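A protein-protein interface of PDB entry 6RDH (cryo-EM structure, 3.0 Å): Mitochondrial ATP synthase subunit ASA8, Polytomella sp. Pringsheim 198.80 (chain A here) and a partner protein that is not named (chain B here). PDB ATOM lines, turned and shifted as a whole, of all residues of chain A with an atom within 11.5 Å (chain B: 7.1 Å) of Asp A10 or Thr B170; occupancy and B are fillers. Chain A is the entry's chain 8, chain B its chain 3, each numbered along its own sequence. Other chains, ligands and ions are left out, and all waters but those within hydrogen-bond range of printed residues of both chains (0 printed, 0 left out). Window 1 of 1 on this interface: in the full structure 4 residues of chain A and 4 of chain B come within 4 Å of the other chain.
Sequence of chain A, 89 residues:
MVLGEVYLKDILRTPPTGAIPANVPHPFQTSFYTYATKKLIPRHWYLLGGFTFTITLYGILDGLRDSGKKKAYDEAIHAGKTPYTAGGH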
ATOM      1  N   LEU A   3     -14.006  17.320  41.683  1.00  0.00           N
ATOM      2  CA  LEU A   3     -14.511  16.576  40.541  1.00  0.00           C
ATOM      3  C   LEU A   3     -14.850  17.587  39.457  1.00  0.00           C
ATOM      4  O   LEU A   3     -15.748  18.413  39.633  1.00  0.00           O
ATOM      5  CB  LEU A   3     -15.716  15.738  40.947  1.00  0.00           C
ATOM      6  CG  LEU A   3     -16.032  14.506  40.113  1.00  0.00           C
ATOM      7  CD1 LEU A   3     -16.647  13.496  41.020  1.00  0.00           C
ATOM      8  CD2 LEU A   3     -16.969  14.800  38.991  1.00  0.00           C
ATOM      9  N   GLY A   4     -14.128  17.529  38.346  1.00  0.00           N
ATOM     10  CA  GLY A   4     -13.957  18.702  37.519  1.00  0.00           C
ATOM     11  C   GLY A   4     -14.367  18.642  36.065  1.00  0.00           C
ATOM     12  O   GLY A   4     -13.580  19.057  35.207  1.00  0.00           O
ATOM     13  N   GLU A   5     -15.523  18.033  35.771  1.00  0.00           N
ATOM     14  CA  GLU A   5     -16.226  18.103  34.485  1.00  0.00           C
ATOM     15  C   GLU A   5     -15.529  17.353  33.356  1.00  0.00           C
ATOM     16  O   GLU A   5     -16.038  17.314  32.234  1.00  0.00           O
ATOM     17  CB  GLU A   5     -16.464  19.559  34.075  1.00  0.00           C
ATOM     18  CG  GLU A   5     -17.748  19.823  33.336  1.00  0.00           C
ATOM     19  CD  GLU A   5     -17.817  21.237  32.796  1.00  0.00           C
ATOM     20  OE1 GLU A   5     -17.089  22.108  33.309  1.00  0.00           O
ATOM     21  OE2 GLU A   5     -18.594  21.479  31.853  1.00  0.00           O
ATOM     22  N   VAL A   6     -14.370  16.758  33.621  1.00  0.00           N
ATOM     23  CA  VAL A   6     -13.782  15.808  32.692  1.00  0.00           C
ATOM     24  C   VAL A   6     -14.001  14.386  33.151  1.00  0.00           C
ATOM     25  O   VAL A   6     -13.740  13.449  32.382  1.00  0.00           O
ATOM     26  CB  VAL A   6     -12.280  16.071  32.482  1.00  0.00           C
ATOM     27  CG1 VAL A   6     -12.064  17.513  32.094  1.00  0.00           C
ATOM     28  CG2 VAL A   6     -11.497  15.721  33.726  1.00  0.00           C
ATOM     29  N   TYR A   7     -14.460  14.190  34.381  1.00  0.00           N
ATOM     30  CA  TYR A   7     -14.964  12.896  34.785  1.00  0.00           C
ATOM     31  C   TYR A   7     -16.407  12.710  34.354  1.00  0.00           C
ATOM     32  O   TYR A   7     -16.873  11.573  34.271  1.00  0.00           O
ATOM     33  CB  TYR A   7     -14.824  12.730  36.297  1.00  0.00           C
ATOM     34  CG  TYR A   7     -13.405  12.897  36.780  1.00  0.00           C
ATOM     35  CD1 TYR A   7     -12.502  11.852  36.698  1.00  0.00           C
ATOM     36  CD2 TYR A   7     -12.966  14.100  37.304  1.00  0.00           C
ATOM     37  CE1 TYR A   7     -11.206  12.001  37.124  1.00  0.00           C
ATOM     38  CE2 TYR A   7     -11.674  14.258  37.737  1.00  0.00           C
ATOM     39  CZ  TYR A   7     -10.797  13.208  37.643  1.00  0.00           C
ATOM     40  OH  TYR A   7      -9.502  13.361  38.077  1.00  0.00           O
ATOM     41  N   LEU A   8     -17.108  13.800  34.060  1.00  0.00           N
ATOM     42  CA  LEU A   8     -18.464  13.760  33.544  1.00  0.00           C
ATOM     43  C   LEU A   8     -18.526  13.853  32.033  1.00  0.00           C
ATOM     44  O   LEU A   8     -19.607  14.078  31.490  1.00  0.00           O
ATOM     45  CB  LEU A   8     -19.287  14.903  34.121  1.00  0.00           C
ATOM     46  CG  LEU A   8     -19.562  15.092  35.597  1.00  0.00           C
ATOM     47  CD1 LEU A   8     -20.522  16.206  35.672  1.00  0.00           C
ATOM     48  CD2 LEU A   8     -20.189  13.891  36.154  1.00  0.00           C
ATOM     49  N   LYS A   9     -17.407  13.734  31.338  1.00  0.00           N
ATOM     50  CA  LYS A   9     -17.415  13.908  29.895  1.00  0.00           C
ATOM     51  C   LYS A   9     -17.908  12.635  29.229  1.00  0.00           C
ATOM     52  O   LYS A   9     -17.382  11.550  29.491  1.00  0.00           O
ATOM     53  CB  LYS A   9     -16.028  14.273  29.387  1.00  0.00           C
ATOM     54  CG  LYS A   9     -16.034  14.863  28.004  1.00  0.00           C
ATOM     55  CD  LYS A   9     -14.664  15.359  27.620  1.00  0.00           C
ATOM     56  CE  LYS A   9     -13.680  14.211  27.477  1.00  0.00           C
ATOM     57  NZ  LYS A   9     -14.007  13.321  26.331  1.00  0.00           N
ATOM     58  N   ASP A  10     -18.947  12.779  28.401  1.00  0.00           N
ATOM     59  CA  ASP A  10     -19.620  11.710  27.662  1.00  0.00           C
ATOM     60  C   ASP A  10     -20.224  10.645  28.565  1.00  0.00           C
ATOM     61  O   ASP A  10     -20.489   9.537  28.111  1.00  0.00           O
ATOM     62  CB  ASP A  10     -18.693  11.045  26.640  1.00  0.00           C
ATOM     63  CG  ASP A  10     -18.180  12.009  25.598  1.00  0.00           C
ATOM     64  OD1 ASP A  10     -18.885  12.990  25.291  1.00  0.00           O
ATOM     65  OD2 ASP A  10     -17.071  11.779  25.077  1.00  0.00           O
ATOM     66  N   ILE A  11     -20.463  10.952  29.832  1.00  0.00           N
ATOM     67  CA  ILE A  11     -21.027   9.993  30.768  1.00  0.00           C
ATOM     68  C   ILE A  11     -22.328  10.553  31.303  1.00  0.00           C
ATOM     69  O   ILE A  11     -23.393   9.950  31.147  1.00  0.00           O
ATOM     70  CB  ILE A  11     -20.066   9.696  31.926  1.00  0.00           C
ATOM     71  CG1 ILE A  11     -18.771   9.093  31.412  1.00  0.00           C
ATOM     72  CG2 ILE A  11     -20.696   8.756  32.882  1.00  0.00           C
ATOM     73  CD1 ILE A  11     -17.753   8.902  32.463  1.00  0.00           C
ATOM     74  N   LEU A  12     -22.245  11.709  31.944  1.00  0.00           N
ATOM     75  CA  LEU A  12     -23.396  12.372  32.534  1.00  0.00           C
ATOM     76  C   LEU A  12     -23.486  13.763  31.947  1.00  0.00           C
ATOM     77  O   LEU A  12     -22.534  14.538  32.042  1.00  0.00           O
ATOM     78  CB  LEU A  12     -23.270  12.459  34.053  1.00  0.00           C
ATOM     79  CG  LEU A  12     -23.537  11.198  34.856  1.00  0.00           C
ATOM     80  CD1 LEU A  12     -23.097  11.418  36.265  1.00  0.00           C
ATOM     81  CD2 LEU A  12     -24.990  10.872  34.813  1.00  0.00           C
ATOM     82  N   ARG A  13     -24.617  14.083  31.343  1.00  0.00           N
ATOM     83  CA  ARG A  13     -24.864  15.429  30.870  1.00  0.00           C
ATOM     84  C   ARG A  13     -26.127  15.962  31.524  1.00  0.00           C
ATOM     85  O   ARG A  13     -26.941  15.208  32.052  1.00  0.00           O
ATOM     86  CB  ARG A  13     -24.989  15.471  29.352  1.00  0.00           C
ATOM     87  CG  ARG A  13     -23.850  14.801  28.626  1.00  0.00           C
ATOM     88  CD  ARG A  13     -23.787  15.251  27.200  1.00  0.00           C
ATOM     89  NE  ARG A  13     -22.678  14.650  26.477  1.00  0.00           N
ATOM     90  CZ  ARG A  13     -22.779  13.568  25.721  1.00  0.00           C
ATOM     91  NH1 ARG A  13     -21.718  13.100  25.096  1.00  0.00           N
ATOM     92  NH2 ARG A  13     -23.937  12.954  25.592  1.00  0.00           N
ATOM     93  N   THR A  14     -26.265  17.266  31.505  1.00  0.00           N
ATOM     94  CA  THR A  14     -27.414  17.977  32.029  1.00  0.00           C
ATOM     95  C   THR A  14     -28.381  18.276  30.896  1.00  0.00           C
ATOM     96  O   THR A  14     -28.046  18.069  29.728  1.00  0.00           O
ATOM     97  CB  THR A  14     -26.940  19.254  32.709  1.00  0.00           C
ATOM     98  OG1 THR A  14     -26.140  19.990  31.787  1.00  0.00           O
ATOM     99  CG2 THR A  14     -26.137  18.912  33.923  1.00  0.00           C
ATOM    100  N   VAL A  24     -30.085  10.215  18.735  1.00  0.00           N
ATOM    101  CA  VAL A  24     -29.027   9.248  18.465  1.00  0.00           C
ATOM    102  C   VAL A  24     -29.637   8.045  17.765  1.00  0.00           C
ATOM    103  O   VAL A  24     -30.550   7.410  18.310  1.00  0.00           O
ATOM    104  CB  VAL A  24     -28.317   8.826  19.753  1.00  0.00           C
ATOM    105  CG1 VAL A  24     -27.416   7.661  19.491  1.00  0.00           C
ATOM    106  CG2 VAL A  24     -27.528   9.963  20.295  1.00  0.00           C
ATOM    107  N   THR B 137     -14.650   4.532  16.537  1.00  0.00           N
ATOM    108  CA  THR B 137     -14.275   3.352  17.300  1.00  0.00           C
ATOM    109  C   THR B 137     -14.084   2.161  16.385  1.00  0.00           C
ATOM    110  O   THR B 137     -13.187   1.341  16.610  1.00  0.00           O
ATOM    111  CB  THR B 137     -15.331   3.033  18.352  1.00  0.00           C
ATOM    112  OG1 THR B 137     -16.404   2.309  17.746  1.00  0.00           O
ATOM    113  CG2 THR B 137     -15.888   4.313  18.928  1.00  0.00           C
ATOM    114  N   VAL B 165      -8.251   5.320  22.368  1.00  0.00           N
ATOM    115  CA  VAL B 165      -9.103   4.510  23.230  1.00  0.00           C
ATOM    116  C   VAL B 165      -9.306   5.202  24.568  1.00  0.00           C
ATOM    117  O   VAL B 165     -10.425   5.278  25.078  1.00  0.00           O
ATOM    118  CB  VAL B 165      -8.516   3.101  23.407  1.00  0.00           C
ATOM    119  CG1 VAL B 165      -9.328   2.309  24.399  1.00  0.00           C
ATOM    120  CG2 VAL B 165      -8.483   2.382  22.089  1.00  0.00           C
ATOM    121  N   SER B 166      -8.242   5.754  25.142  1.00  0.00           N
ATOM    122  CA  SER B 166      -8.354   6.373  26.451  1.00  0.00           C
ATOM    123  C   SER B 166      -9.076   7.709  26.412  1.00  0.00           C
ATOM    124  O   SER B 166      -9.577   8.151  27.447  1.00  0.00           O
ATOM    125  CB  SER B 166      -6.967   6.558  27.050  1.00  0.00           C
ATOM    126  OG  SER B 166      -7.053   7.205  28.304  1.00  0.00           O
ATOM    127  N   ALA B 167      -9.148   8.364  25.259  1.00  0.00           N
ATOM    128  CA  ALA B 167      -9.898   9.606  25.177  1.00  0.00           C
ATOM    129  C   ALA B 167     -11.351   9.395  24.799  1.00  0.00           C
ATOM    130  O   ALA B 167     -12.161  10.307  24.984  1.00  0.00           O
ATOM    131  CB  ALA B 167      -9.256  10.558  24.170  1.00  0.00           C
ATOM    132  N   ASN B 168     -11.700   8.226  24.270  1.00  0.00           N
ATOM    133  CA  ASN B 168     -13.068   7.890  23.898  1.00  0.00           C
ATOM    134  C   ASN B 168     -13.436   6.522  24.430  1.00  0.00           C
ATOM    135  O   ASN B 168     -13.962   5.682  23.709  1.00  0.00           O
ATOM    136  CB  ASN B 168     -13.270   7.887  22.392  1.00  0.00           C
ATOM    137  CG  ASN B 168     -12.698   9.091  21.725  1.00  0.00           C
ATOM    138  OD1 ASN B 168     -13.277  10.170  21.763  1.00  0.00           O
ATOM    139  ND2 ASN B 168     -11.559   8.917  21.085  1.00  0.00           N
ATOM    140  N   PHE B 169     -13.155   6.264  25.702  1.00  0.00           N
ATOM    141  CA  PHE B 169     -13.427   4.939  26.240  1.00  0.00           C
ATOM    142  C   PHE B 169     -14.911   4.695  26.458  1.00  0.00           C
ATOM    143  O   PHE B 169     -15.333   3.542  26.505  1.00  0.00           O
ATOM    144  CB  PHE B 169     -12.641   4.730  27.532  1.00  0.00           C
ATOM    145  CG  PHE B 169     -13.255   5.372  28.732  1.00  0.00           C
ATOM    146  CD1 PHE B 169     -13.247   6.739  28.885  1.00  0.00           C
ATOM    147  CD2 PHE B 169     -13.814   4.598  29.727  1.00  0.00           C
ATOM    148  CE1 PHE B 169     -13.809   7.314  29.980  1.00  0.00           C
ATOM    149  CE2 PHE B 169     -14.371   5.174  30.823  1.00  0.00           C
ATOM    150  CZ  PHE B 169     -14.368   6.531  30.949  1.00  0.00           C
ATOM    151  N   THR B 170     -15.717   5.745  26.539  1.00  0.00           N
ATOM    152  CA  THR B 170     -17.146   5.558  26.716  1.00  0.00           C
ATOM    153  C   THR B 170     -17.838   5.114  25.441  1.00  0.00           C
ATOM    154  O   THR B 170     -18.978   4.655  25.506  1.00  0.00           O
ATOM    155  CB  THR B 170     -17.781   6.846  27.212  1.00  0.00           C
ATOM    156  OG1 THR B 170     -17.300   7.935  26.428  1.00  0.00           O
ATOM    157  CG2 THR B 170     -17.416   7.087  28.630  1.00  0.00           C
ATOM    158  N   LYS B 171     -17.184   5.231  24.291  1.00  0.00           N
ATOM    159  CA  LYS B 171     -17.813   4.944  23.013  1.00  0.00           C
ATOM    160  C   LYS B 171     -17.452   3.584  22.456  1.00  0.00           C
ATOM    161  O   LYS B 171     -17.971   3.206  21.408  1.00  0.00           O
ATOM    162  CB  LYS B 171     -17.449   6.012  21.995  1.00  0.00           C
ATOM    163  CG  LYS B 171     -17.875   7.382  22.405  1.00  0.00           C
ATOM    164  CD  LYS B 171     -17.716   8.352  21.277  1.00  0.00           C
ATOM    165  CE  LYS B 171     -17.855   9.752  21.787  1.00  0.00           C
ATOM    166  NZ  LYS B 171     -16.915   9.972  22.914  1.00  0.00           N
ATOM    167  N   PHE B 172     -16.581   2.843  23.115  1.00  0.00           N
ATOM    168  CA  PHE B 172     -16.175   1.530  22.651  1.00  0.00           C
ATOM    169  C   PHE B 172     -17.085   0.479  23.256  1.00  0.00           C
ATOM    170  O   PHE B 172     -17.460   0.570  24.425  1.00  0.00           O
ATOM    171  CB  PHE B 172     -14.727   1.245  23.040  1.00  0.00           C
ATOM    172  CG  PHE B 172     -13.733   1.771  22.070  1.00  0.00           C
ATOM    173  CD1 PHE B 172     -13.183   0.949  21.113  1.00  0.00           C
ATOM    174  CD2 PHE B 172     -13.364   3.090  22.101  1.00  0.00           C
ATOM    175  CE1 PHE B 172     -12.288   1.438  20.218  1.00  0.00           C
ATOM    176  CE2 PHE B 172     -12.473   3.589  21.206  1.00  0.00           C
ATOM    177  CZ  PHE B 172     -11.928   2.765  20.267  1.00  0.00           C
ATOM    178  N   GLU B 173     -17.445  -0.514  22.465  1.00  0.00           N
ATOM    179  CA  GLU B 173     -18.169  -1.643  23.015  1.00  0.00           C
ATOM    180  C   GLU B 173     -17.211  -2.800  23.233  1.00  0.00           C
ATOM    181  O   GLU B 173     -16.066  -2.771  22.794  1.00  0.00           O
ATOM    182  CB  GLU B 173     -19.349  -2.045  22.125  1.00  0.00           C
ATOM    183  CG  GLU B 173     -19.106  -2.014  20.647  1.00  0.00           C
ATOM    184  CD  GLU B 173     -19.872  -0.896  19.974  1.00  0.00           C
ATOM    185  OE1 GLU B 173     -20.351   0.006  20.684  1.00  0.00           O
ATOM    186  OE2 GLU B 173     -20.013  -0.926  18.735  1.00  0.00           O
ATOM    187  N   ASP B 197      -8.781   2.538  31.797  1.00  0.00           N
ATOM    188  CA  ASP B 197      -9.858   3.008  30.936  1.00  0.00           C
ATOM    189  C   ASP B 197     -10.565   1.867  30.224  1.00  0.00           C
ATOM    190  O   ASP B 197     -11.783   1.923  30.053  1.00  0.00           O
ATOM    191  CB  ASP B 197      -9.323   4.009  29.924  1.00  0.00           C
ATOM    192  CG  ASP B 197      -8.979   5.330  30.556  1.00  0.00           C
ATOM    193  OD1 ASP B 197      -9.642   5.701  31.544  1.00  0.00           O
ATOM    194  OD2 ASP B 197      -8.054   6.004  30.069  1.00  0.00           O
ATOM    195  N   SER B 201     -14.422   0.962  30.796  1.00  0.00           N
ATOM    196  CA  SER B 201     -15.320   0.887  29.656  1.00  0.00           C
ATOM    197  C   SER B 201     -16.092  -0.422  29.636  1.00  0.00           C
ATOM    198  O   SER B 201     -17.320  -0.414  29.528  1.00  0.00           O
ATOM    199  CB  SER B 201     -14.529   1.058  28.377  1.00  0.00           C
ATOM    200  OG  SER B 201     -15.396   1.036  27.268  1.00  0.00           O
ATOM    201  N   CYS B 205     -19.296   1.248  30.924  1.00  0.00           N
ATOM    202  CA  CYS B 205     -19.763   1.920  29.729  1.00  0.00           C
ATOM    203  C   CYS B 205     -20.410   0.979  28.736  1.00  0.00           C
ATOM    204  O   CYS B 205     -20.895   1.439  27.703  1.00  0.00           O
ATOM    205  CB  CYS B 205     -18.607   2.646  29.056  1.00  0.00           C
ATOM    206  SG  CYS B 205     -17.743   3.755  30.143  1.00  0.00           S
ATOM    207  N   ASN B 206     -20.413  -0.318  29.005  1.00  0.00           N
ATOM    208  CA  ASN B 206     -20.989  -1.303  28.110  1.00  0.00           C
ATOM    209  C   ASN B 206     -21.992  -2.138  28.877  1.00  0.00           C
ATOM    210  O   ASN B 206     -22.077  -2.069  30.102  1.00  0.00           O
ATOM    211  CB  ASN B 206     -19.918  -2.196  27.494  1.00  0.00           C
ATOM    212  CG  ASN B 206     -18.980  -1.435  26.604  1.00  0.00           C
ATOM    213  OD1 ASN B 206     -17.820  -1.783  26.466  1.00  0.00           O
ATOM    214  ND2 ASN B 206     -19.472  -0.383  26.004  1.00  0.00           N
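NZ of Lys A9 lies within salt-bridge range of OD2 of Asp A10, 3.7 Å away. OD1 of Asp A10 lies within salt-bridge range of NH1 of Arg A13 (2.8 Å).
O of Ala B167 touches NZ of Lys A9, 3.8 Å away. OG1 of Thr B170 touches CB of Asp A10 (3.4 Å). Thr B170 touches Ile A11 (CG2 to CG1, 3.7 Å).
Of chain A, only Asp A10 (3.4 Å) and Ile A11 (3.7 Å) come within 4 Å of Thr B170. Asn B168 touches none of the printed residues of chain A. No residue of chain A comes within 4 Å of Phe B169. Of the printed residues of chain A, Lys B171 touches Asp A10. No residue of chain A comes within 4 Å of Ser B201. No residue of chain A comes within 4 Å of Cys B205. Printed residues of chain B within 4 Å of Lys A9: Ala B167 (3.8 Å). Printed residues of chain B within 4 Å of Ile A11: Thr B170. Of the printed residues of chain A, Ala B167 touches Lys A9 (3.8 Å). Leu A8 touches none of the printed residues of chain B. The nearest residue of chain B that does not touch Asp A10 is Ala B167 (5.1 Å).
OD2 of Asp A10 is in salt-bridge range of NZ of Lys B171 (2.8 Å).
Hydrophobic or aromatic side chains of chain A within 4 Å of the printed part of chain B: Ile A11. Along chain A the printed residues that touch a printed residue of chain B span positions 9 to 11. Among the printed residues, 4 pairs touch across the chains. Among the printed residues, Asp or Glu carboxylates within 4 Å of a Lys or Arg side-chain nitrogen of the other chain: Asp A10 with Lys B171.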
